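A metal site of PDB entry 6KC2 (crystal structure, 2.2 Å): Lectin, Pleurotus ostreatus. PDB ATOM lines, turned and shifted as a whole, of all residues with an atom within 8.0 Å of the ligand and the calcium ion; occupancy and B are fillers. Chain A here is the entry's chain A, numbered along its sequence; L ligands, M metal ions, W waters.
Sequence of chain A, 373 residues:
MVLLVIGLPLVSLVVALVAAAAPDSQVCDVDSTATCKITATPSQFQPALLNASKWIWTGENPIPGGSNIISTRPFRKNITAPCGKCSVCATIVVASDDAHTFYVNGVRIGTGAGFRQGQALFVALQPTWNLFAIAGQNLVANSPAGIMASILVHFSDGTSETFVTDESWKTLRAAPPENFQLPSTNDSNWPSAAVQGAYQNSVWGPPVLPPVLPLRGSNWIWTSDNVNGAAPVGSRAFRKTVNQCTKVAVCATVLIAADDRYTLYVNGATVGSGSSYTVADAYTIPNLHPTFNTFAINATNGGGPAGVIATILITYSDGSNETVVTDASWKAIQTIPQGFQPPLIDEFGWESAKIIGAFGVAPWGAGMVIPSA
O2 of the ligand is in hydrogen-bond range of OH of Tyr 277 (2.8 Å).
Hydrophobic or aromatic side chains within 4 Å of the ligand: Tyr 277 and Pro 305. Five residues have an atom within 4 Å of the ligand: Asp 259, Asp 260, Tyr 277, Gly 303 and Pro 305.
N of Gly 302 sits close to OD2 of Asp 260 (2.6 Å). The backbone carbonyl oxygen (O) of Gly 304 lies within hydrogen-bond range of the side-chain amide nitrogen (ND2) of Asn 301 (3.0 Å). O of Ala 231 is in hydrogen-bond range of ND2 of Asn 301 (2.9 Å). The backbone carbonyl oxygen (O) of Pro 232 is in hydrogen-bond range of the side-chain amide nitrogen (ND2) of Asn 301 (3.1 Å). NE1 of Trp 364 is in hydrogen-bond range of OD2 of Asp 259. The backbone NH (N) of Asp 259 is in hydrogen-bond range of the backbone carbonyl oxygen (O) of Gly 307, 2.5 Å away.
The calcium ion is bound by the backbone carbonyl oxygen (O) of Pro 305 (2.3 Å). The calcium ion is bound by the side-chain carboxylate (OD2) of Asp 260 (2.4 Å). The calcium ion is bound by the side-chain amide oxygen (OD1) of Asn 301 (2.5 Å). O4 of the ligand binds the calcium ion (2.6 Å). The calcium ion is bound by an oxygen (O3) of the ligand (2.6 Å). O of Gly 303 binds the calcium ion (2.6 Å). The calcium ion is bound by OD1 of Asp 259. The calcium ion has seven donor atoms within binding distance.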
ATOM      1  N   TRP A 222      -7.509  -9.906 -12.720  1.00  0.00           N
ATOM      2  CA  TRP A 222      -7.958 -10.718 -11.591  1.00  0.00           C
ATOM      3  C   TRP A 222      -8.524  -9.785 -10.514  1.00  0.00           C
ATOM      4  O   TRP A 222      -8.503  -8.560 -10.652  1.00  0.00           O
ATOM      5  CB  TRP A 222      -6.825 -11.593 -11.048  1.00  0.00           C
ATOM      6  CG  TRP A 222      -7.285 -12.835 -10.327  1.00  0.00           C
ATOM      7  CD1 TRP A 222      -7.203 -13.095  -8.989  1.00  0.00           C
ATOM      8  CD2 TRP A 222      -7.899 -13.995 -10.927  1.00  0.00           C
ATOM      9  NE1 TRP A 222      -7.727 -14.334  -8.706  1.00  0.00           N
ATOM     10  CE2 TRP A 222      -8.162 -14.913  -9.880  1.00  0.00           C
ATOM     11  CE3 TRP A 222      -8.256 -14.350 -12.226  1.00  0.00           C
ATOM     12  CZ2 TRP A 222      -8.762 -16.144 -10.099  1.00  0.00           C
ATOM     13  CZ3 TRP A 222      -8.847 -15.585 -12.455  1.00  0.00           C
ATOM     14  CH2 TRP A 222      -9.089 -16.478 -11.389  1.00  0.00           C
ATOM     15  N   GLY A 229       2.694 -12.221  -7.775  1.00  0.00           N
ATOM     16  CA  GLY A 229       2.725 -13.304  -8.727  1.00  0.00           C
ATOM     17  C   GLY A 229       1.896 -14.518  -8.383  1.00  0.00           C
ATOM     18  O   GLY A 229       2.037 -15.562  -9.036  1.00  0.00           O
ATOM     19  N   ALA A 230       1.037 -14.437  -7.366  1.00  0.00           N
ATOM     20  CA  ALA A 230       0.179 -15.556  -7.032  1.00  0.00           C
ATOM     21  C   ALA A 230      -1.128 -15.013  -6.468  1.00  0.00           C
ATOM     22  O   ALA A 230      -1.212 -13.857  -6.039  1.00  0.00           O
ATOM     23  CB  ALA A 230       0.836 -16.529  -6.037  1.00  0.00           C
ATOM     24  N   ALA A 231      -2.146 -15.848  -6.484  1.00  0.00           N
ATOM     25  CA  ALA A 231      -3.448 -15.471  -5.965  1.00  0.00           C
ATOM     26  C   ALA A 231      -3.990 -16.648  -5.173  1.00  0.00           C
ATOM     27  O   ALA A 231      -3.600 -17.795  -5.421  1.00  0.00           O
ATOM     28  CB  ALA A 231      -4.435 -15.090  -7.076  1.00  0.00           C
ATOM     29  N   PRO A 232      -4.891 -16.398  -4.223  1.00  0.00           N
ATOM     30  CA  PRO A 232      -5.486 -17.496  -3.457  1.00  0.00           C
ATOM     31  C   PRO A 232      -6.184 -18.498  -4.354  1.00  0.00           C
ATOM     32  O   PRO A 232      -6.625 -18.185  -5.463  1.00  0.00           O
ATOM     33  CB  PRO A 232      -6.475 -16.787  -2.531  1.00  0.00           C
ATOM     34  CG  PRO A 232      -5.915 -15.408  -2.380  1.00  0.00           C
ATOM     35  CD  PRO A 232      -5.258 -15.074  -3.684  1.00  0.00           C
ATOM     36  N   VAL A 233      -6.285 -19.741  -3.870  1.00  0.00           N
ATOM     37  CA  VAL A 233      -7.144 -20.713  -4.519  1.00  0.00           C
ATOM     38  C   VAL A 233      -8.592 -20.254  -4.383  1.00  0.00           C
ATOM     39  O   VAL A 233      -9.006 -19.767  -3.328  1.00  0.00           O
ATOM     40  CB  VAL A 233      -6.951 -22.112  -3.894  1.00  0.00           C
ATOM     41  CG1 VAL A 233      -7.870 -23.140  -4.557  1.00  0.00           C
ATOM     42  CG2 VAL A 233      -5.487 -22.538  -4.007  1.00  0.00           C
ATOM     43  N   ALA A 258      -8.169 -18.418 -19.402  1.00  0.00           N
ATOM     44  CA  ALA A 258      -8.016 -18.120 -17.980  1.00  0.00           C
ATOM     45  C   ALA A 258      -6.959 -19.007 -17.344  1.00  0.00           C
ATOM     46  O   ALA A 258      -6.884 -20.217 -17.616  1.00  0.00           O
ATOM     47  CB  ALA A 258      -9.337 -18.274 -17.223  1.00  0.00           C
ATOM     48  N   ASP A 259      -6.157 -18.417 -16.465  1.00  0.00           N
ATOM     49  CA  ASP A 259      -5.221 -19.272 -15.753  1.00  0.00           C
ATOM     50  C   ASP A 259      -6.025 -20.054 -14.755  1.00  0.00           C
ATOM     51  O   ASP A 259      -6.468 -19.539 -13.716  1.00  0.00           O
ATOM     52  CB  ASP A 259      -4.074 -18.533 -15.069  1.00  0.00           C
ATOM     53  CG  ASP A 259      -3.130 -19.503 -14.319  1.00  0.00           C
ATOM     54  OD1 ASP A 259      -3.583 -20.580 -13.864  1.00  0.00           O
ATOM     55  OD2 ASP A 259      -1.917 -19.222 -14.238  1.00  0.00           O
ATOM     56  N   ASP A 260      -6.107 -21.336 -15.112  1.00  0.00           N
ATOM     57  CA  ASP A 260      -6.783 -22.495 -14.583  1.00  0.00           C
ATOM     58  C   ASP A 260      -8.097 -22.629 -15.343  1.00  0.00           C
ATOM     59  O   ASP A 260      -8.106 -23.436 -16.272  1.00  0.00           O
ATOM     60  CB  ASP A 260      -6.808 -22.477 -13.065  1.00  0.00           C
ATOM     61  CG  ASP A 260      -5.426 -22.861 -12.512  1.00  0.00           C
ATOM     62  OD1 ASP A 260      -4.706 -23.580 -13.243  1.00  0.00           O
ATOM     63  OD2 ASP A 260      -5.039 -22.401 -11.419  1.00  0.00           O
ATOM     64  N   ARG A 261      -9.141 -21.852 -15.077  1.00  0.00           N
ATOM     65  CA  ARG A 261     -10.398 -22.185 -15.767  1.00  0.00           C
ATOM     66  C   ARG A 261     -11.408 -21.042 -15.687  1.00  0.00           C
ATOM     67  O   ARG A 261     -11.287 -20.147 -14.856  1.00  0.00           O
ATOM     68  CB  ARG A 261     -11.020 -23.478 -15.221  1.00  0.00           C
ATOM     69  CG  ARG A 261     -11.378 -23.435 -13.734  1.00  0.00           C
ATOM     70  CD  ARG A 261     -11.652 -24.818 -13.150  1.00  0.00           C
ATOM     71  NE  ARG A 261     -12.434 -25.641 -14.066  1.00  0.00           N
ATOM     72  CZ  ARG A 261     -12.035 -26.812 -14.572  1.00  0.00           C
ATOM     73  NH1 ARG A 261     -10.849 -27.309 -14.222  1.00  0.00           N
ATOM     74  NH2 ARG A 261     -12.823 -27.481 -15.410  1.00  0.00           N
ATOM     75  N   TYR A 277      -4.846 -22.210 -20.045  1.00  0.00           N
ATOM     76  CA  TYR A 277      -4.271 -20.892 -20.260  1.00  0.00           C
ATOM     77  C   TYR A 277      -3.231 -20.900 -21.377  1.00  0.00           C
ATOM     78  O   TYR A 277      -2.541 -19.897 -21.574  1.00  0.00           O
ATOM     79  CB  TYR A 277      -3.684 -20.344 -18.950  1.00  0.00           C
ATOM     80  CG  TYR A 277      -2.686 -21.251 -18.243  1.00  0.00           C
ATOM     81  CD1 TYR A 277      -1.344 -21.266 -18.628  1.00  0.00           C
ATOM     82  CD2 TYR A 277      -3.067 -22.065 -17.180  1.00  0.00           C
ATOM     83  CE1 TYR A 277      -0.410 -22.072 -17.983  1.00  0.00           C
ATOM     84  CE2 TYR A 277      -2.147 -22.891 -16.531  1.00  0.00           C
ATOM     85  CZ  TYR A 277      -0.817 -22.881 -16.936  1.00  0.00           C
ATOM     86  OH  TYR A 277       0.137 -23.667 -16.319  1.00  0.00           O
ATOM     87  N   THR A 300     -11.573 -19.532 -12.028  1.00  0.00           N
ATOM     88  CA  THR A 300     -11.157 -20.256 -10.846  1.00  0.00           C
ATOM     89  C   THR A 300      -9.651 -20.446 -10.857  1.00  0.00           C
ATOM     90  O   THR A 300      -9.083 -20.857 -11.871  1.00  0.00           O
ATOM     91  CB  THR A 300     -11.852 -21.611 -10.764  1.00  0.00           C
ATOM     92  OG1 THR A 300     -13.274 -21.425 -10.822  1.00  0.00           O
ATOM     93  CG2 THR A 300     -11.474 -22.347  -9.474  1.00  0.00           C
ATOM     94  N   ASN A 301      -9.003 -20.159  -9.736  1.00  0.00           N
ATOM     95  CA  ASN A 301      -7.573 -20.424  -9.583  1.00  0.00           C
ATOM     96  C   ASN A 301      -7.376 -21.699  -8.764  1.00  0.00           C
ATOM     97  O   ASN A 301      -7.836 -21.779  -7.619  1.00  0.00           O
ATOM     98  CB  ASN A 301      -6.853 -19.252  -8.923  1.00  0.00           C
ATOM     99  CG  ASN A 301      -5.349 -19.527  -8.779  1.00  0.00           C
ATOM    100  OD1 ASN A 301      -4.786 -20.282  -9.568  1.00  0.00           O
ATOM    101  ND2 ASN A 301      -4.730 -18.951  -7.774  1.00  0.00           N
ATOM    102  N   GLY A 302      -6.661 -22.664  -9.344  1.00  0.00           N
ATOM    103  CA  GLY A 302      -6.336 -23.903  -8.649  1.00  0.00           C
ATOM    104  C   GLY A 302      -5.074 -23.837  -7.803  1.00  0.00           C
ATOM    105  O   GLY A 302      -4.763 -24.826  -7.111  1.00  0.00           O
ATOM    106  N   GLY A 303      -4.368 -22.719  -7.832  1.00  0.00           N
ATOM    107  CA  GLY A 303      -3.144 -22.528  -7.083  1.00  0.00           C
ATOM    108  C   GLY A 303      -2.110 -21.759  -7.900  1.00  0.00           C
ATOM    109  O   GLY A 303      -2.034 -21.930  -9.114  1.00  0.00           O
ATOM    110  N   GLY A 304      -1.330 -20.917  -7.247  1.00  0.00           N
ATOM    111  CA  GLY A 304      -0.286 -20.177  -7.918  1.00  0.00           C
ATOM    112  C   GLY A 304      -0.826 -18.945  -8.607  1.00  0.00           C
ATOM    113  O   GLY A 304      -1.808 -18.339  -8.157  1.00  0.00           O
ATOM    114  N   PRO A 305      -0.183 -18.546  -9.701  1.00  0.00           N
ATOM    115  CA  PRO A 305      -0.653 -17.388 -10.478  1.00  0.00           C
ATOM    116  C   PRO A 305      -2.075 -17.589 -10.978  1.00  0.00           C
ATOM    117  O   PRO A 305      -2.582 -18.710 -11.104  1.00  0.00           O
ATOM    118  CB  PRO A 305       0.338 -17.312 -11.658  1.00  0.00           C
ATOM    119  CG  PRO A 305       1.566 -18.078 -11.196  1.00  0.00           C
ATOM    120  CD  PRO A 305       1.027 -19.168 -10.294  1.00  0.00           C
ATOM    121  N   ALA A 306      -2.732 -16.460 -11.265  1.00  0.00           N
ATOM    122  CA  ALA A 306      -4.094 -16.506 -11.795  1.00  0.00           C
ATOM    123  C   ALA A 306      -4.329 -15.291 -12.686  1.00  0.00           C
ATOM    124  O   ALA A 306      -3.722 -14.231 -12.498  1.00  0.00           O
ATOM    125  CB  ALA A 306      -5.139 -16.553 -10.664  1.00  0.00           C
ATOM    126  N   GLY A 307      -5.242 -15.462 -13.634  1.00  0.00           N
ATOM    127  CA  GLY A 307      -5.639 -14.369 -14.519  1.00  0.00           C
ATOM    128  C   GLY A 307      -6.674 -14.869 -15.509  1.00  0.00           C
ATOM    129  O   GLY A 307      -6.773 -16.058 -15.797  1.00  0.00           O
ATOM    130  N   ALA A 362       5.143 -12.596 -18.452  1.00  0.00           N
ATOM    131  CA  ALA A 362       5.318 -13.787 -17.633  1.00  0.00           C
ATOM    132  C   ALA A 362       4.204 -13.861 -16.573  1.00  0.00           C
ATOM    133  O   ALA A 362       3.735 -12.828 -16.090  1.00  0.00           O
ATOM    134  CB  ALA A 362       6.695 -13.747 -16.950  1.00  0.00           C
ATOM    135  N   PRO A 363       3.802 -15.067 -16.174  1.00  0.00           N
ATOM    136  CA  PRO A 363       4.375 -16.353 -16.573  1.00  0.00           C
ATOM    137  C   PRO A 363       3.800 -16.957 -17.842  1.00  0.00           C
ATOM    138  O   PRO A 363       4.360 -17.953 -18.315  1.00  0.00           O
ATOM    139  CB  PRO A 363       4.040 -17.255 -15.380  1.00  0.00           C
ATOM    140  CG  PRO A 363       2.702 -16.702 -14.876  1.00  0.00           C
ATOM    141  CD  PRO A 363       2.827 -15.201 -15.067  1.00  0.00           C
ATOM    142  N   TRP A 364       2.718 -16.396 -18.386  1.00  0.00           N
ATOM    143  CA  TRP A 364       2.030 -17.066 -19.497  1.00  0.00           C
ATOM    144  C   TRP A 364       2.679 -16.787 -20.847  1.00  0.00           C
ATOM    145  O   TRP A 364       2.571 -17.614 -21.750  1.00  0.00           O
ATOM    146  CB  TRP A 364       0.555 -16.661 -19.524  1.00  0.00           C
ATOM    147  CG  TRP A 364      -0.084 -16.776 -18.163  1.00  0.00           C
ATOM    148  CD1 TRP A 364      -0.440 -17.930 -17.517  1.00  0.00           C
ATOM    149  CD2 TRP A 364      -0.394 -15.703 -17.269  1.00  0.00           C
ATOM    150  NE1 TRP A 364      -0.954 -17.632 -16.269  1.00  0.00           N
ATOM    151  CE2 TRP A 364      -0.945 -16.275 -16.101  1.00  0.00           C
ATOM    152  CE3 TRP A 364      -0.259 -14.298 -17.349  1.00  0.00           C
ATOM    153  CZ2 TRP A 364      -1.372 -15.506 -15.009  1.00  0.00           C
ATOM    154  CZ3 TRP A 364      -0.686 -13.529 -16.257  1.00  0.00           C
ATOM    155  CH2 TRP A 364      -1.239 -14.132 -15.099  1.00  0.00           C
HETATM  156  C1  LIG L   1       1.386 -24.172 -12.750  1.00  0.00           C
HETATM  157  C2  LIG L   1      -0.121 -24.395 -12.633  1.00  0.00           C
HETATM  158  C3  LIG L   1      -0.823 -23.114 -12.191  1.00  0.00           C
HETATM  159  C4  LIG L   1      -0.378 -21.935 -13.070  1.00  0.00           C
HETATM  160  C5  LIG L   1       1.157 -21.895 -13.225  1.00  0.00           C
HETATM  161  C6  LIG L   1       1.620 -20.777 -14.164  1.00  0.00           C
HETATM  162  O1  LIG L   1       1.943 -23.831 -11.483  1.00  0.00           O
HETATM  163  O2  LIG L   1      -0.630 -24.789 -13.887  1.00  0.00           O
HETATM  164  O3  LIG L   1      -2.233 -23.268 -12.198  1.00  0.00           O
HETATM  165  O4  LIG L   1      -0.813 -20.749 -12.464  1.00  0.00           O
HETATM  166  O5  LIG L   1       1.632 -23.142 -13.685  1.00  0.00           O
HETATM  167 CA    CA M   1      -3.122 -20.978 -11.307  1.00  0.00          CA
HETATM  168  O   HOH W   1      -2.934 -25.069  -9.948  1.00  0.00           O
